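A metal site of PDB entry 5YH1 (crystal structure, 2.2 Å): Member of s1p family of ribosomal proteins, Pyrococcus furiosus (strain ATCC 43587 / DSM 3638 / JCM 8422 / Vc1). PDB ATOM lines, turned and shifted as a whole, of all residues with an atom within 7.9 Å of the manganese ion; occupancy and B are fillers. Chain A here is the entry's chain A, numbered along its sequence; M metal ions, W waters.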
ATOM      1  N   HIS A  63     -21.172  -9.718  -5.915  1.00  0.00           N
ATOM      2  CA  HIS A  63     -22.172  -9.415  -4.899  1.00  0.00           C
ATOM      3  C   HIS A  63     -23.580  -9.552  -5.497  1.00  0.00           C
ATOM      4  O   HIS A  63     -23.786  -9.251  -6.685  1.00  0.00           O
ATOM      5  CB  HIS A  63     -21.956  -8.015  -4.343  1.00  0.00           C
ATOM      6  CG  HIS A  63     -22.804  -7.713  -3.156  1.00  0.00           C
ATOM      7  ND1 HIS A  63     -23.779  -6.737  -3.167  1.00  0.00           N
ATOM      8  CD2 HIS A  63     -22.847  -8.272  -1.923  1.00  0.00           C
ATOM      9  CE1 HIS A  63     -24.377  -6.704  -1.997  1.00  0.00           C
ATOM     10  NE2 HIS A  63     -23.830  -7.626  -1.221  1.00  0.00           N
ATOM     11  N   ASP A  65     -26.513  -8.082  -5.629  1.00  0.00           N
ATOM     12  CA  ASP A  65     -27.477  -6.999  -5.790  1.00  0.00           C
ATOM     13  C   ASP A  65     -27.452  -6.476  -7.212  1.00  0.00           C
ATOM     14  O   ASP A  65     -26.727  -7.008  -8.065  1.00  0.00           O
ATOM     15  CB  ASP A  65     -27.258  -5.895  -4.737  1.00  0.00           C
ATOM     16  CG  ASP A  65     -25.944  -5.156  -4.895  1.00  0.00           C
ATOM     17  OD1 ASP A  65     -25.131  -5.455  -5.798  1.00  0.00           O
ATOM     18  OD2 ASP A  65     -25.706  -4.261  -4.066  1.00  0.00           O
ATOM     19  N   THR A  66     -28.258  -5.457  -7.487  1.00  0.00           N
ATOM     20  CA  THR A  66     -28.430  -4.987  -8.852  1.00  0.00           C
ATOM     21  C   THR A  66     -27.095  -4.623  -9.499  1.00  0.00           C
ATOM     22  O   THR A  66     -26.802  -5.079 -10.601  1.00  0.00           O
ATOM     23  CB  THR A  66     -29.433  -3.813  -8.922  1.00  0.00           C
ATOM     24  OG1 THR A  66     -30.759  -4.304  -8.654  1.00  0.00           O
ATOM     25  CG2 THR A  66     -29.424  -3.156 -10.304  1.00  0.00           C
ATOM     26  N   ASP A  67     -26.292  -3.842  -8.795  1.00  0.00           N
ATOM     27  CA  ASP A  67     -24.977  -3.407  -9.321  1.00  0.00           C
ATOM     28  C   ASP A  67     -24.069  -4.608  -9.590  1.00  0.00           C
ATOM     29  O   ASP A  67     -23.453  -4.724 -10.649  1.00  0.00           O
ATOM     30  CB  ASP A  67     -24.336  -2.425  -8.342  1.00  0.00           C
ATOM     31  CG  ASP A  67     -23.003  -1.865  -8.836  1.00  0.00           C
ATOM     32  OD1 ASP A  67     -22.906  -1.439 -10.001  1.00  0.00           O
ATOM     33  OD2 ASP A  67     -22.035  -1.845  -8.027  1.00  0.00           O
ATOM     34  N   GLY A  68     -24.023  -5.530  -8.628  1.00  0.00           N
ATOM     35  CA  GLY A  68     -23.217  -6.747  -8.769  1.00  0.00           C
ATOM     36  C   GLY A  68     -23.661  -7.684  -9.872  1.00  0.00           C
ATOM     37  O   GLY A  68     -22.828  -8.161 -10.646  1.00  0.00           O
ATOM     38  N   ALA A  71     -22.900  -6.038 -13.205  1.00  0.00           N
ATOM     39  CA  ALA A  71     -21.470  -6.124 -13.465  1.00  0.00           C
ATOM     40  C   ALA A  71     -21.082  -7.526 -13.909  1.00  0.00           C
ATOM     41  O   ALA A  71     -20.384  -7.702 -14.920  1.00  0.00           O
ATOM     42  CB  ALA A  71     -20.690  -5.727 -12.225  1.00  0.00           C
ATOM     43  N   VAL A 136     -16.130  -9.285  -8.296  1.00  0.00           N
ATOM     44  CA  VAL A 136     -16.752  -8.064  -8.797  1.00  0.00           C
ATOM     45  C   VAL A 136     -17.771  -7.538  -7.803  1.00  0.00           C
ATOM     46  O   VAL A 136     -18.614  -8.305  -7.291  1.00  0.00           O
ATOM     47  CB  VAL A 136     -17.455  -8.333 -10.141  1.00  0.00           C
ATOM     48  CG1 VAL A 136     -18.101  -7.073 -10.684  1.00  0.00           C
ATOM     49  CG2 VAL A 136     -16.456  -8.900 -11.143  1.00  0.00           C
ATOM     50  N   ASP A 137     -17.699  -6.239  -7.526  1.00  0.00           N
ATOM     51  CA  ASP A 137     -18.506  -5.570  -6.502  1.00  0.00           C
ATOM     52  C   ASP A 137     -18.244  -6.061  -5.072  1.00  0.00           C
ATOM     53  O   ASP A 137     -18.919  -5.684  -4.116  1.00  0.00           O
ATOM     54  CB  ASP A 137     -20.010  -5.634  -6.840  1.00  0.00           C
ATOM     55  CG  ASP A 137     -20.821  -4.593  -6.093  1.00  0.00           C
ATOM     56  OD1 ASP A 137     -20.360  -3.424  -5.992  1.00  0.00           O
ATOM     57  OD2 ASP A 137     -21.893  -4.944  -5.565  1.00  0.00           O
ATOM     58  N   ASN A 138     -17.225  -6.902  -4.953  1.00  0.00           N
ATOM     59  CA  ASN A 138     -16.706  -7.409  -3.687  1.00  0.00           C
ATOM     60  C   ASN A 138     -15.218  -7.537  -3.965  1.00  0.00           C
ATOM     61  O   ASN A 138     -14.801  -7.397  -5.113  1.00  0.00           O
ATOM     62  CB  ASN A 138     -17.267  -8.809  -3.385  1.00  0.00           C
ATOM     63  CG  ASN A 138     -18.546  -8.794  -2.569  1.00  0.00           C
ATOM     64  OD1 ASN A 138     -19.036  -7.747  -2.180  1.00  0.00           O
ATOM     65  ND2 ASN A 138     -19.081  -9.995  -2.308  1.00  0.00           N
ATOM     66  N   ASP A 162     -13.953  -3.577  -8.168  1.00  0.00           N
ATOM     67  CA  ASP A 162     -14.770  -3.179  -7.034  1.00  0.00           C
ATOM     68  C   ASP A 162     -14.718  -1.652  -6.865  1.00  0.00           C
ATOM     69  O   ASP A 162     -13.867  -0.985  -7.464  1.00  0.00           O
ATOM     70  CB  ASP A 162     -14.267  -3.919  -5.777  1.00  0.00           C
ATOM     71  CG  ASP A 162     -15.238  -3.881  -4.630  1.00  0.00           C
ATOM     72  OD1 ASP A 162     -16.403  -3.421  -4.805  1.00  0.00           O
ATOM     73  OD2 ASP A 162     -14.834  -4.318  -3.514  1.00  0.00           O
ATOM     74  N   HIS A 163     -15.622  -1.102  -6.060  1.00  0.00           N
ATOM     75  CA  HIS A 163     -15.654   0.350  -5.795  1.00  0.00           C
ATOM     76  C   HIS A 163     -15.888   0.693  -4.325  1.00  0.00           C
ATOM     77  O   HIS A 163     -16.232   1.839  -3.999  1.00  0.00           O
ATOM     78  CB  HIS A 163     -16.715   1.027  -6.672  1.00  0.00           C
ATOM     79  CG  HIS A 163     -18.110   0.592  -6.376  1.00  0.00           C
ATOM     80  ND1 HIS A 163     -19.105   1.476  -5.987  1.00  0.00           N
ATOM     81  CD2 HIS A 163     -18.682  -0.635  -6.387  1.00  0.00           C
ATOM     82  CE1 HIS A 163     -20.225   0.808  -5.790  1.00  0.00           C
ATOM     83  NE2 HIS A 163     -19.998  -0.467  -6.025  1.00  0.00           N
ATOM     84  N   HIS A 164     -15.663  -0.283  -3.450  1.00  0.00           N
ATOM     85  CA  HIS A 164     -15.647  -0.055  -2.010  1.00  0.00           C
ATOM     86  C   HIS A 164     -14.249   0.352  -1.576  1.00  0.00           C
ATOM     87  O   HIS A 164     -13.256  -0.003  -2.232  1.00  0.00           O
ATOM     88  CB  HIS A 164     -16.106  -1.312  -1.263  1.00  0.00           C
ATOM     89  CG  HIS A 164     -17.509  -1.715  -1.594  1.00  0.00           C
ATOM     90  ND1 HIS A 164     -17.817  -2.456  -2.711  1.00  0.00           N
ATOM     91  CD2 HIS A 164     -18.683  -1.417  -0.993  1.00  0.00           C
ATOM     92  CE1 HIS A 164     -19.128  -2.619  -2.773  1.00  0.00           C
ATOM     93  NE2 HIS A 164     -19.676  -1.993  -1.743  1.00  0.00           N
ATOM     94  N   TYR A 195     -16.818   6.366  -4.491  1.00  0.00           N
ATOM     95  CA  TYR A 195     -17.714   5.197  -4.514  1.00  0.00           C
ATOM     96  C   TYR A 195     -18.728   5.233  -5.656  1.00  0.00           C
ATOM     97  O   TYR A 195     -19.216   4.192  -6.085  1.00  0.00           O
ATOM     98  CB  TYR A 195     -18.464   5.136  -3.178  1.00  0.00           C
ATOM     99  CG  TYR A 195     -19.556   4.076  -3.089  1.00  0.00           C
ATOM    100  CD1 TYR A 195     -19.257   2.766  -2.733  1.00  0.00           C
ATOM    101  CD2 TYR A 195     -20.890   4.397  -3.353  1.00  0.00           C
ATOM    102  CE1 TYR A 195     -20.252   1.793  -2.648  1.00  0.00           C
ATOM    103  CE2 TYR A 195     -21.891   3.430  -3.273  1.00  0.00           C
ATOM    104  CZ  TYR A 195     -21.566   2.139  -2.906  1.00  0.00           C
ATOM    105  OH  TYR A 195     -22.532   1.162  -2.820  1.00  0.00           O
ATOM    106  N   LEU A 197     -18.621   5.769  -8.759  1.00  0.00           N
ATOM    107  CA  LEU A 197     -18.321   5.007  -9.977  1.00  0.00           C
ATOM    108  C   LEU A 197     -18.421   3.517  -9.623  1.00  0.00           C
ATOM    109  O   LEU A 197     -17.500   2.937  -9.024  1.00  0.00           O
ATOM    110  CB  LEU A 197     -16.926   5.361 -10.515  1.00  0.00           C
ATOM    111  CG  LEU A 197     -16.537   4.785 -11.876  1.00  0.00           C
ATOM    112  CD1 LEU A 197     -17.438   5.302 -12.980  1.00  0.00           C
ATOM    113  CD2 LEU A 197     -15.092   5.116 -12.158  1.00  0.00           C
ATOM    114  N   THR A 198     -19.542   2.914  -9.985  1.00  0.00           N
ATOM    115  CA  THR A 198     -19.943   1.608  -9.430  1.00  0.00           C
ATOM    116  C   THR A 198     -19.405   0.416 -10.224  1.00  0.00           C
ATOM    117  O   THR A 198     -18.899   0.563 -11.346  1.00  0.00           O
ATOM    118  CB  THR A 198     -21.484   1.506  -9.342  1.00  0.00           C
ATOM    119  OG1 THR A 198     -22.038   1.299 -10.645  1.00  0.00           O
ATOM    120  CG2 THR A 198     -22.060   2.765  -8.730  1.00  0.00           C
ATOM    121  N   ALA A 199     -19.550  -0.771  -9.658  1.00  0.00           N
ATOM    122  CA  ALA A 199     -18.961  -1.980 -10.247  1.00  0.00           C
ATOM    123  C   ALA A 199     -19.500  -2.263 -11.634  1.00  0.00           C
ATOM    124  O   ALA A 199     -18.752  -2.685 -12.515  1.00  0.00           O
ATOM    125  CB  ALA A 199     -19.182  -3.185  -9.340  1.00  0.00           C
ATOM    126  N   GLY A 200     -20.786  -2.022 -11.837  1.00  0.00           N
ATOM    127  CA  GLY A 200     -21.415  -2.234 -13.139  1.00  0.00           C
ATOM    128  C   GLY A 200     -20.901  -1.276 -14.215  1.00  0.00           C
ATOM    129  O   GLY A 200     -20.854  -1.621 -15.391  1.00  0.00           O
ATOM    130  N   ALA A 225     -27.021  -0.361 -13.323  1.00  0.00           N
ATOM    131  CA  ALA A 225     -26.148  -0.538 -12.153  1.00  0.00           C
ATOM    132  C   ALA A 225     -26.122   0.681 -11.264  1.00  0.00           C
ATOM    133  O   ALA A 225     -26.289   0.581 -10.041  1.00  0.00           O
ATOM    134  CB  ALA A 225     -24.738  -0.894 -12.606  1.00  0.00           C
ATOM    135  N   GLY A 228     -29.345   1.054  -9.394  1.00  0.00           N
ATOM    136  CA  GLY A 228     -29.322   0.137  -8.252  1.00  0.00           C
ATOM    137  C   GLY A 228     -28.559   0.673  -7.058  1.00  0.00           C
ATOM    138  O   GLY A 228     -29.060   0.631  -5.932  1.00  0.00           O
ATOM    139  N   ASP A 229     -27.352   1.184  -7.305  1.00  0.00           N
ATOM    140  CA  ASP A 229     -26.485   1.719  -6.242  1.00  0.00           C
ATOM    141  C   ASP A 229     -26.719   3.199  -5.931  1.00  0.00           C
ATOM    142  O   ASP A 229     -26.021   3.751  -5.078  1.00  0.00           O
ATOM    143  CB  ASP A 229     -25.009   1.515  -6.613  1.00  0.00           C
ATOM    144  CG  ASP A 229     -24.423   0.216  -6.069  1.00  0.00           C
ATOM    145  OD1 ASP A 229     -25.169  -0.650  -5.552  1.00  0.00           O
ATOM    146  OD2 ASP A 229     -23.191   0.075  -6.178  1.00  0.00           O
ATOM    147  N   HIS A 410     -19.917   2.181   5.054  1.00  0.00           N
ATOM    148  CA  HIS A 410     -19.712   3.575   4.681  1.00  0.00           C
ATOM    149  C   HIS A 410     -19.768   4.424   5.923  1.00  0.00           C
ATOM    150  O   HIS A 410     -20.251   3.973   6.970  1.00  0.00           O
ATOM    151  CB  HIS A 410     -20.789   4.053   3.705  1.00  0.00           C
ATOM    152  CG  HIS A 410     -20.854   3.238   2.463  1.00  0.00           C
ATOM    153  ND1 HIS A 410     -19.991   3.421   1.407  1.00  0.00           N
ATOM    154  CD2 HIS A 410     -21.676   2.215   2.099  1.00  0.00           C
ATOM    155  CE1 HIS A 410     -20.277   2.551   0.453  1.00  0.00           C
ATOM    156  NE2 HIS A 410     -21.289   1.812   0.845  1.00  0.00           N
HETATM  157 MN    MN M   1     -21.987  -1.781  -5.914  1.00  0.00          MN
HETATM  158  O   HOH W   1     -23.596  -3.126  -5.335  1.00  0.00           O
HETATM  159  O   HOH W   2     -22.157  -1.293  -3.751  1.00  0.00           O
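Water W2 lies within hydrogen-bond range of OH of Tyr 195 (2.7 Å) and NE2 of His 164 (3.3 Å).
Of the 21 residues printed, 4 come within 4 Å of the manganese ion.
The nearest printed residue that does not touch the manganese ion is Tyr 195 (4.3 Å).
OD1 of Asp 67 lies within hydrogen-bond range of N of Ala 199 (3.4 Å).
The side-chain hydroxyl (OG1) of Thr 198 sits at hydrogen-bond distance from the side-chain carboxylate (OD1) of Asp 67.
The side-chain carboxylate (OD1) of Asp 67 sits at hydrogen-bond distance from the backbone NH (N) of Gly 200 (2.9 Å).
ND1 of His 163 sits at hydrogen-bond distance from O of Tyr 195, at 2.7 Å.
The manganese ion is bound by the side-chain carboxylate (OD2) of Asp 67 (2.1 Å), water W1 (2.2 Å), water W2 (2.2 Å), the side-chain carboxylate (OD2) of Asp 229 (2.2 Å), the side-chain carboxylate (OD1) of Asp 137 (2.3 Å) and a ring nitrogen (NE2) of His 163 (2.4 Å).
The manganese ion has six donor atoms within binding distance.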
